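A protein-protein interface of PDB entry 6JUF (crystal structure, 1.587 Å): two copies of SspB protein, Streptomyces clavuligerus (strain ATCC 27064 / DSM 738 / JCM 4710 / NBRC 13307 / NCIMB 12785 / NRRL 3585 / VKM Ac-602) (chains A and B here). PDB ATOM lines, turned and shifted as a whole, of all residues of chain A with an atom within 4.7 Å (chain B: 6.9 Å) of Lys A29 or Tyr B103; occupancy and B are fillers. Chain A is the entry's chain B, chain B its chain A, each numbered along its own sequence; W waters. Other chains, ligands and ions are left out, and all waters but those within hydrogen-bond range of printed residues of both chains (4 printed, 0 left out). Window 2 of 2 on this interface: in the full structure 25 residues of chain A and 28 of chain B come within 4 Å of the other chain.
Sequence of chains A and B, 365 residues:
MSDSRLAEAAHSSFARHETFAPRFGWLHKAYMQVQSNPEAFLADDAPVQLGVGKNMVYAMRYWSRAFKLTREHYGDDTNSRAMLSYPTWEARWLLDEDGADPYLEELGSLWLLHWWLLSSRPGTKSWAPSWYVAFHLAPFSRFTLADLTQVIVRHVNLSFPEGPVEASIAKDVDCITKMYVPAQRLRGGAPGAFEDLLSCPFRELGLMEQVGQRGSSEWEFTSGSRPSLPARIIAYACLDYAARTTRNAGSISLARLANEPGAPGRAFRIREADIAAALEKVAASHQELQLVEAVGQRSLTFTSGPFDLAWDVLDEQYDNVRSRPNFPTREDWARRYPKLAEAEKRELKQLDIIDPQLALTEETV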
ATOM      1  N   PHE A  24      23.636   3.559  -5.873  1.00  0.00           N
ATOM      2  CA  PHE A  24      23.651   2.438  -6.813  1.00  0.00           C
ATOM      3  C   PHE A  24      22.727   2.716  -8.016  1.00  0.00           C
ATOM      4  O   PHE A  24      23.155   2.540  -9.179  1.00  0.00           O
ATOM      5  CB  PHE A  24      23.216   1.118  -6.174  1.00  0.00           C
ATOM      6  CG  PHE A  24      22.952   0.070  -7.217  1.00  0.00           C
ATOM      7  CD1 PHE A  24      24.050  -0.518  -7.892  1.00  0.00           C
ATOM      8  CD2 PHE A  24      21.633  -0.255  -7.641  1.00  0.00           C
ATOM      9  CE1 PHE A  24      23.845  -1.382  -8.965  1.00  0.00           C
ATOM     10  CE2 PHE A  24      21.454  -1.158  -8.675  1.00  0.00           C
ATOM     11  CZ  PHE A  24      22.565  -1.711  -9.332  1.00  0.00           C
ATOM     12  N   GLY A  25      21.502   3.207  -7.763  1.00  0.00           N
ATOM     13  CA  GLY A  25      20.526   3.361  -8.895  1.00  0.00           C
ATOM     14  C   GLY A  25      21.055   4.331  -9.958  1.00  0.00           C
ATOM     15  O   GLY A  25      20.850   4.176 -11.155  1.00  0.00           O
ATOM     16  N   TRP A  26      21.831   5.308  -9.514  1.00  0.00           N
ATOM     17  CA  TRP A  26      22.484   6.228 -10.455  1.00  0.00           C
ATOM     18  C   TRP A  26      23.492   5.567 -11.318  1.00  0.00           C
ATOM     19  O   TRP A  26      23.572   5.890 -12.522  1.00  0.00           O
ATOM     20  CB  TRP A  26      23.161   7.328  -9.668  1.00  0.00           C
ATOM     21  CG  TRP A  26      22.178   8.295  -9.091  1.00  0.00           C
ATOM     22  CD1 TRP A  26      20.785   8.237  -9.129  1.00  0.00           C
ATOM     23  CD2 TRP A  26      22.506   9.494  -8.369  1.00  0.00           C
ATOM     24  NE1 TRP A  26      20.231   9.317  -8.471  1.00  0.00           N
ATOM     25  CE2 TRP A  26      21.241  10.121  -8.006  1.00  0.00           C
ATOM     26  CE3 TRP A  26      23.737  10.128  -8.030  1.00  0.00           C
ATOM     27  CZ2 TRP A  26      21.187  11.332  -7.326  1.00  0.00           C
ATOM     28  CZ3 TRP A  26      23.675  11.357  -7.314  1.00  0.00           C
ATOM     29  CH2 TRP A  26      22.408  11.942  -6.966  1.00  0.00           C
ATOM     30  N   LEU A  27      24.349   4.695 -10.742  1.00  0.00           N
ATOM     31  CA  LEU A  27      25.355   4.014 -11.541  1.00  0.00           C
ATOM     32  C   LEU A  27      24.715   3.108 -12.601  1.00  0.00           C
ATOM     33  O   LEU A  27      25.141   3.110 -13.773  1.00  0.00           O
ATOM     34  CB  LEU A  27      26.342   3.236 -10.655  1.00  0.00           C
ATOM     35  CG  LEU A  27      27.069   4.080  -9.590  1.00  0.00           C
ATOM     36  CD1 LEU A  27      27.893   3.086  -8.756  1.00  0.00           C
ATOM     37  CD2 LEU A  27      27.951   5.136 -10.226  1.00  0.00           C
ATOM     38  N   HIS A  28      23.696   2.377 -12.146  1.00  0.00           N
ATOM     39  CA  HIS A  28      22.901   1.417 -12.978  1.00  0.00           C
ATOM     40  C   HIS A  28      22.205   2.093 -14.131  1.00  0.00           C
ATOM     41  O   HIS A  28      22.444   1.772 -15.320  1.00  0.00           O
ATOM     42  CB  HIS A  28      21.932   0.742 -12.066  1.00  0.00           C
ATOM     43  CG  HIS A  28      21.077  -0.312 -12.768  1.00  0.00           C
ATOM     44  ND1 HIS A  28      21.594  -1.478 -13.247  1.00  0.00           N
ATOM     45  CD2 HIS A  28      19.724  -0.352 -13.026  1.00  0.00           C
ATOM     46  CE1 HIS A  28      20.599  -2.218 -13.785  1.00  0.00           C
ATOM     47  NE2 HIS A  28      19.469  -1.562 -13.643  1.00  0.00           N
ATOM     48  N   LYS A  29      21.417   3.100 -13.793  1.00  0.00           N
ATOM     49  CA  LYS A  29      20.648   3.856 -14.814  1.00  0.00           C
ATOM     50  C   LYS A  29      21.525   4.639 -15.781  1.00  0.00           C
ATOM     51  O   LYS A  29      21.227   4.693 -17.009  1.00  0.00           O
ATOM     52  CB  LYS A  29      19.610   4.731 -14.125  1.00  0.00           C
ATOM     53  CG  LYS A  29      18.481   3.856 -13.580  1.00  0.00           C
ATOM     54  CD  LYS A  29      17.246   4.616 -13.138  1.00  0.00           C
ATOM     55  CE  LYS A  29      17.543   5.490 -11.943  1.00  0.00           C
ATOM     56  NZ  LYS A  29      16.428   6.436 -11.618  1.00  0.00           N
ATOM     57  N   ALA A  30      22.633   5.221 -15.294  1.00  0.00           N
ATOM     58  CA  ALA A  30      23.561   5.859 -16.235  1.00  0.00           C
ATOM     59  C   ALA A  30      24.086   4.900 -17.267  1.00  0.00           C
ATOM     60  O   ALA A  30      24.113   5.255 -18.460  1.00  0.00           O
ATOM     61  CB  ALA A  30      24.702   6.605 -15.520  1.00  0.00           C
ATOM     62  N   TYR A  31      24.515   3.682 -16.856  1.00  0.00           N
ATOM     63  CA  TYR A  31      25.088   2.767 -17.806  1.00  0.00           C
ATOM     64  C   TYR A  31      24.042   2.388 -18.823  1.00  0.00           C
ATOM     65  O   TYR A  31      24.318   2.351 -20.035  1.00  0.00           O
ATOM     66  CB  TYR A  31      25.667   1.489 -17.112  1.00  0.00           C
ATOM     67  CG  TYR A  31      26.094   0.416 -18.115  1.00  0.00           C
ATOM     68  CD1 TYR A  31      27.270   0.536 -18.864  1.00  0.00           C
ATOM     69  CD2 TYR A  31      25.235  -0.665 -18.399  1.00  0.00           C
ATOM     70  CE1 TYR A  31      27.642  -0.412 -19.824  1.00  0.00           C
ATOM     71  CE2 TYR A  31      25.613  -1.637 -19.344  1.00  0.00           C
ATOM     72  CZ  TYR A  31      26.812  -1.502 -20.052  1.00  0.00           C
ATOM     73  OH  TYR A  31      27.161  -2.461 -20.970  1.00  0.00           O
ATOM     74  N   MET A  32      22.845   2.068 -18.321  1.00  0.00           N
ATOM     75  CA  MET A  32      21.766   1.522 -19.148  1.00  0.00           C
ATOM     76  C   MET A  32      21.351   2.513 -20.245  1.00  0.00           C
ATOM     77  O   MET A  32      21.126   2.147 -21.420  1.00  0.00           O
ATOM     78  CB  MET A  32      20.579   1.013 -18.297  1.00  0.00           C
ATOM     79  CG  MET A  32      20.846  -0.308 -17.545  1.00  0.00           C
ATOM     80  SD  MET A  32      21.615  -1.772 -18.381  1.00  0.00           S
ATOM     81  CE  MET A  32      20.433  -2.085 -19.699  1.00  0.00           C
ATOM     82  N   GLN A  33      21.343   3.769 -19.871  1.00  0.00           N
ATOM     83  CA  GLN A  33      21.008   4.818 -20.856  1.00  0.00           C
ATOM     84  C   GLN A  33      22.103   5.272 -21.788  1.00  0.00           C
ATOM     85  O   GLN A  33      21.848   5.489 -22.994  1.00  0.00           O
ATOM     86  CB  GLN A  33      20.425   6.024 -20.149  1.00  0.00           C
ATOM     87  CG  GLN A  33      19.136   5.630 -19.426  1.00  0.00           C
ATOM     88  CD  GLN A  33      18.013   6.609 -19.671  1.00  0.00           C
ATOM     89  OE1 GLN A  33      18.166   7.604 -20.401  1.00  0.00           O
ATOM     90  NE2 GLN A  33      16.867   6.339 -19.055  1.00  0.00           N
ATOM     91  N   LEU A  50      15.795   9.688 -16.854  1.00  0.00           N
ATOM     92  CA  LEU A  50      16.686   9.026 -15.929  1.00  0.00           C
ATOM     93  C   LEU A  50      15.986   8.836 -14.590  1.00  0.00           C
ATOM     94  O   LEU A  50      16.476   8.069 -13.719  1.00  0.00           O
ATOM     95  CB  LEU A  50      18.000   9.830 -15.758  1.00  0.00           C
ATOM     96  CG  LEU A  50      18.906   9.966 -16.973  1.00  0.00           C
ATOM     97  CD1 LEU A  50      19.865  11.134 -16.744  1.00  0.00           C
ATOM     98  CD2 LEU A  50      19.649   8.668 -17.301  1.00  0.00           C
ATOM     99  N   GLY A  51      14.868   9.550 -14.413  1.00  0.00           N
ATOM    100  CA  GLY A  51      14.061   9.458 -13.209  1.00  0.00           C
ATOM    101  C   GLY A  51      14.726  10.094 -12.022  1.00  0.00           C
ATOM    102  O   GLY A  51      14.814   9.477 -10.963  1.00  0.00           O
ATOM    103  N   VAL A  52      15.190  11.333 -12.185  1.00  0.00           N
ATOM    104  CA  VAL A  52      15.842  12.076 -11.108  1.00  0.00           C
ATOM    105  C   VAL A  52      15.626  13.599 -11.340  1.00  0.00           C
ATOM    106  O   VAL A  52      15.214  13.998 -12.416  1.00  0.00           O
ATOM    107  CB  VAL A  52      17.376  11.789 -11.060  1.00  0.00           C
ATOM    108  CG1 VAL A  52      17.704  10.321 -10.898  1.00  0.00           C
ATOM    109  CG2 VAL A  52      18.046  12.263 -12.352  1.00  0.00           C
ATOM    110  N   PHE B  24      20.184  -6.796  -2.674  1.00  0.00           N
ATOM    111  CA  PHE B  24      19.284  -5.978  -3.442  1.00  0.00           C
ATOM    112  C   PHE B  24      18.940  -6.612  -4.824  1.00  0.00           C
ATOM    113  O   PHE B  24      17.793  -6.665  -5.240  1.00  0.00           O
ATOM    114  CB  PHE B  24      19.845  -4.558  -3.685  1.00  0.00           C
ATOM    115  CG  PHE B  24      19.092  -3.811  -4.732  1.00  0.00           C
ATOM    116  CD1 PHE B  24      17.785  -3.358  -4.479  1.00  0.00           C
ATOM    117  CD2 PHE B  24      19.606  -3.672  -6.034  1.00  0.00           C
ATOM    118  CE1 PHE B  24      17.028  -2.760  -5.494  1.00  0.00           C
ATOM    119  CE2 PHE B  24      18.852  -3.031  -7.019  1.00  0.00           C
ATOM    120  CZ  PHE B  24      17.559  -2.587  -6.752  1.00  0.00           C
ATOM    121  N   HIS B  28      15.204  -7.239  -6.512  1.00  0.00           N
ATOM    122  CA  HIS B  28      14.886  -6.560  -7.786  1.00  0.00           C
ATOM    123  C   HIS B  28      14.585  -7.478  -8.953  1.00  0.00           C
ATOM    124  O   HIS B  28      13.499  -7.381  -9.590  1.00  0.00           O
ATOM    125  CB  HIS B  28      16.034  -5.601  -8.130  1.00  0.00           C
ATOM    126  CG  HIS B  28      15.912  -4.931  -9.473  1.00  0.00           C
ATOM    127  ND1 HIS B  28      15.074  -3.883  -9.687  1.00  0.00           N
ATOM    128  CD2 HIS B  28      16.597  -5.150 -10.670  1.00  0.00           C
ATOM    129  CE1 HIS B  28      15.202  -3.466 -10.992  1.00  0.00           C
ATOM    130  NE2 HIS B  28      16.149  -4.229 -11.591  1.00  0.00           N
ATOM    131  N   LEU B  94       6.586  -0.659  -4.125  1.00  0.00           N
ATOM    132  CA  LEU B  94       7.938  -0.320  -3.708  1.00  0.00           C
ATOM    133  C   LEU B  94       8.997  -0.470  -4.786  1.00  0.00           C
ATOM    134  O   LEU B  94       9.866   0.419  -4.995  1.00  0.00           O
ATOM    135  CB  LEU B  94       8.338  -1.225  -2.504  1.00  0.00           C
ATOM    136  CG  LEU B  94       9.807  -0.997  -2.040  1.00  0.00           C
ATOM    137  CD1 LEU B  94      10.020   0.418  -1.453  1.00  0.00           C
ATOM    138  CD2 LEU B  94      10.206  -2.082  -1.045  1.00  0.00           C
ATOM    139  N   LEU B  95       8.971  -1.595  -5.490  1.00  0.00           N
ATOM    140  CA  LEU B  95      10.064  -2.006  -6.332  1.00  0.00           C
ATOM    141  C   LEU B  95       9.915  -1.726  -7.819  1.00  0.00           C
ATOM    142  O   LEU B  95      10.905  -1.859  -8.541  1.00  0.00           O
ATOM    143  CB  LEU B  95      10.363  -3.521  -6.138  1.00  0.00           C
ATOM    144  CG  LEU B  95      10.802  -3.871  -4.707  1.00  0.00           C
ATOM    145  CD1 LEU B  95      10.860  -5.407  -4.647  1.00  0.00           C
ATOM    146  CD2 LEU B  95      12.128  -3.224  -4.418  1.00  0.00           C
ATOM    147  N   ASP B  96       8.735  -1.452  -8.309  1.00  0.00           N
ATOM    148  CA  ASP B  96       8.557  -1.179  -9.723  1.00  0.00           C
ATOM    149  C   ASP B  96       9.407   0.025 -10.130  1.00  0.00           C
ATOM    150  O   ASP B  96       9.656   0.953  -9.332  1.00  0.00           O
ATOM    151  CB  ASP B  96       7.099  -0.889  -9.990  1.00  0.00           C
ATOM    152  CG  ASP B  96       6.749  -1.087 -11.434  1.00  0.00           C
ATOM    153  OD1 ASP B  96       6.832  -0.094 -12.194  1.00  0.00           O
ATOM    154  OD2 ASP B  96       6.446  -2.224 -11.816  1.00  0.00           O
ATOM    155  N   GLU B  97       9.863   0.026 -11.372  1.00  0.00           N
ATOM    156  CA  GLU B  97      10.519   1.200 -11.891  1.00  0.00           C
ATOM    157  C   GLU B  97       9.678   2.455 -11.679  1.00  0.00           C
ATOM    158  O   GLU B  97      10.221   3.541 -11.412  1.00  0.00           O
ATOM    159  CB  GLU B  97      10.888   0.980 -13.386  1.00  0.00           C
ATOM    160  CG  GLU B  97      10.516   2.068 -14.367  1.00  0.00           C
ATOM    161  CD  GLU B  97      10.502   1.555 -15.819  1.00  0.00           C
ATOM    162  OE1 GLU B  97       9.868   0.508 -16.119  1.00  0.00           O
ATOM    163  OE2 GLU B  97      11.131   2.210 -16.670  1.00  0.00           O
ATOM    164  N   ALA B 100       7.927   3.417  -5.412  1.00  0.00           N
ATOM    165  CA  ALA B 100       8.371   4.279  -4.355  1.00  0.00           C
ATOM    166  C   ALA B 100       9.880   4.408  -4.328  1.00  0.00           C
ATOM    167  O   ALA B 100      10.420   5.509  -4.180  1.00  0.00           O
ATOM    168  CB  ALA B 100       7.882   3.802  -2.972  1.00  0.00           C
ATOM    169  N   ASP B 101      10.587   3.284  -4.397  1.00  0.00           N
ATOM    170  CA  ASP B 101      12.029   3.338  -4.270  1.00  0.00           C
ATOM    171  C   ASP B 101      12.655   2.060  -4.853  1.00  0.00           C
ATOM    172  O   ASP B 101      13.211   1.233  -4.111  1.00  0.00           O
ATOM    173  CB  ASP B 101      12.380   3.543  -2.779  1.00  0.00           C
ATOM    174  CG  ASP B 101      13.869   3.820  -2.520  1.00  0.00           C
ATOM    175  OD1 ASP B 101      14.638   4.068  -3.454  1.00  0.00           O
ATOM    176  OD2 ASP B 101      14.303   3.842  -1.330  1.00  0.00           O
ATOM    177  N   PRO B 102      12.575   1.904  -6.200  1.00  0.00           N
ATOM    178  CA  PRO B 102      13.041   0.690  -6.876  1.00  0.00           C
ATOM    179  C   PRO B 102      14.513   0.307  -6.575  1.00  0.00           C
ATOM    180  O   PRO B 102      14.882  -0.859  -6.620  1.00  0.00           O
ATOM    181  CB  PRO B 102      12.831   1.024  -8.389  1.00  0.00           C
ATOM    182  CG  PRO B 102      12.654   2.521  -8.416  1.00  0.00           C
ATOM    183  CD  PRO B 102      11.963   2.850  -7.152  1.00  0.00           C
ATOM    184  N   TYR B 103      15.367   1.284  -6.334  1.00  0.00           N
ATOM    185  CA  TYR B 103      16.801   1.026  -6.099  1.00  0.00           C
ATOM    186  C   TYR B 103      17.190   1.166  -4.649  1.00  0.00           C
ATOM    187  O   TYR B 103      18.408   1.223  -4.357  1.00  0.00           O
ATOM    188  CB  TYR B 103      17.683   1.875  -7.059  1.00  0.00           C
ATOM    189  CG  TYR B 103      17.333   1.495  -8.483  1.00  0.00           C
ATOM    190  CD1 TYR B 103      17.808   0.274  -9.022  1.00  0.00           C
ATOM    191  CD2 TYR B 103      16.522   2.314  -9.265  1.00  0.00           C
ATOM    192  CE1 TYR B 103      17.388  -0.121 -10.323  1.00  0.00           C
ATOM    193  CE2 TYR B 103      16.151   1.935 -10.557  1.00  0.00           C
ATOM    194  CZ  TYR B 103      16.590   0.727 -11.059  1.00  0.00           C
ATOM    195  OH  TYR B 103      16.309   0.348 -12.347  1.00  0.00           O
ATOM    196  N   LEU B 104      16.212   1.208  -3.726  1.00  0.00           N
ATOM    197  CA  LEU B 104      16.493   1.296  -2.255  1.00  0.00           C
ATOM    198  C   LEU B 104      17.521   2.386  -1.976  1.00  0.00           C
ATOM    199  O   LEU B 104      18.525   2.186  -1.248  1.00  0.00           O
ATOM    200  CB  LEU B 104      16.907  -0.067  -1.667  1.00  0.00           C
ATOM    201  CG  LEU B 104      15.908  -1.234  -1.901  1.00  0.00           C
ATOM    202  CD1 LEU B 104      16.436  -2.466  -1.162  1.00  0.00           C
ATOM    203  CD2 LEU B 104      14.466  -0.889  -1.468  1.00  0.00           C
ATOM    204  N   GLU B 105      17.265   3.558  -2.540  1.00  0.00           N
ATOM    205  CA  GLU B 105      18.153   4.693  -2.353  1.00  0.00           C
ATOM    206  C   GLU B 105      17.939   5.354  -0.984  1.00  0.00           C
ATOM    207  O   GLU B 105      18.853   6.104  -0.532  1.00  0.00           O
ATOM    208  CB  GLU B 105      17.930   5.806  -3.436  1.00  0.00           C
ATOM    209  CG  GLU B 105      18.217   5.284  -4.807  1.00  0.00           C
ATOM    210  CD  GLU B 105      17.775   6.257  -5.889  1.00  0.00           C
ATOM    211  OE1 GLU B 105      17.868   7.502  -5.658  1.00  0.00           O
ATOM    212  OE2 GLU B 105      17.338   5.768  -6.976  1.00  0.00           O
ATOM    213  N   GLU B 106      16.777   5.155  -0.369  1.00  0.00           N
ATOM    214  CA  GLU B 106      16.467   5.782   0.917  1.00  0.00           C
ATOM    215  C   GLU B 106      16.542   4.751   2.034  1.00  0.00           C
ATOM    216  O   GLU B 106      15.979   3.669   1.947  1.00  0.00           O
ATOM    217  CB  GLU B 106      15.063   6.410   0.875  1.00  0.00           C
ATOM    218  CG  GLU B 106      15.058   7.687   0.062  1.00  0.00           C
ATOM    219  CD  GLU B 106      13.757   8.445   0.182  1.00  0.00           C
ATOM    220  OE1 GLU B 106      13.098   8.415   1.250  1.00  0.00           O
ATOM    221  OE2 GLU B 106      13.391   9.080  -0.836  1.00  0.00           O
HETATM  222  O   HOH W   1      17.510   7.015  -9.195  1.00  0.00           O
HETATM  223  O   HOH W   2      16.888  -2.502 -13.919  1.00  0.00           O
HETATM  224  O   HOH W   3      17.449   9.231  -7.682  1.00  0.00           O
HETATM  225  O   HOH W   4      20.424   3.007  -5.096  1.00  0.00           O
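The side-chain amino group (NZ) of Lys A29 lies within hydrogen-bond range of the backbone carbonyl oxygen (O) of Leu A50.
Phe A24 touches Phe B24.
Phe A24 touches Tyr B103.
CA of Gly A25 touches CB of Tyr B103 (3.7 Å).
Tyr B103 touches His A28 (OH to CD2, 3.6 Å).
Lys A29 touches Tyr B103 (CD to CE2, 3.9 Å).
Tyr B103 touches just these residues of chain A: Phe A24 (3.9 Å), Gly A25 (3.7 Å), His A28 (3.6 Å) and Lys A29 (3.9 Å).
Printed residues of chain B within 4 Å of Phe A24: Phe B24 and Tyr B103.
Of the printed residues of chain B, His A28 touches Tyr B103 (3.6 Å).
Of the printed residues of chain B, Gly A25 touches Tyr B103 (3.7 Å).
Printed residues of chain A within 4 Å of Phe B24: Phe A24 (3.6 Å).
Ala B100 touches none of the printed residues of chain A.
Asp B96 touches none of the printed residues of chain A.
The nearest printed residue of chain A that does not touch Tyr B103 is Trp A26 (5.9 Å).
Printed residues of chain A that touch a printed residue of chain B: Phe A24, Gly A25, His A28 and Lys A29.
Hydrophobic or aromatic side chains of chain A within 4 Å of the printed part of chain B: Phe A24 and His A28.
Hydrophobic or aromatic side chains of chain B within 4 Å of the printed part of chain A: Phe B24 and Tyr B103.
Among the printed residues, no Asp or Glu carboxylate lies within 4 Å of a Lys or Arg side-chain nitrogen of the other chain.
Phe B24 touches its own counterpart, Phe A24.
Positions printed for both chains: 24 and 28.
Water W1 bridges the side-chain carboxylate of Glu B105 (2.6 Å) and the side-chain amino group of Lys A29 (2.7 Å).
Water W3 lies within hydrogen-bond range of OE1 of Glu B105 (2.7 Å) and NE1 of Trp A26 (2.9 Å).
Water W2 lies within hydrogen-bond range of NE2 of His A28 (2.8 Å), NE2 of His B28 (3.0 Å) and OH of Tyr B103 (3.3 Å).
Water W4 lies within hydrogen-bond range of O of Tyr B103 (2.8 Å), N of Gly A25 (2.9 Å) and N of Phe A24 (3.4 Å).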
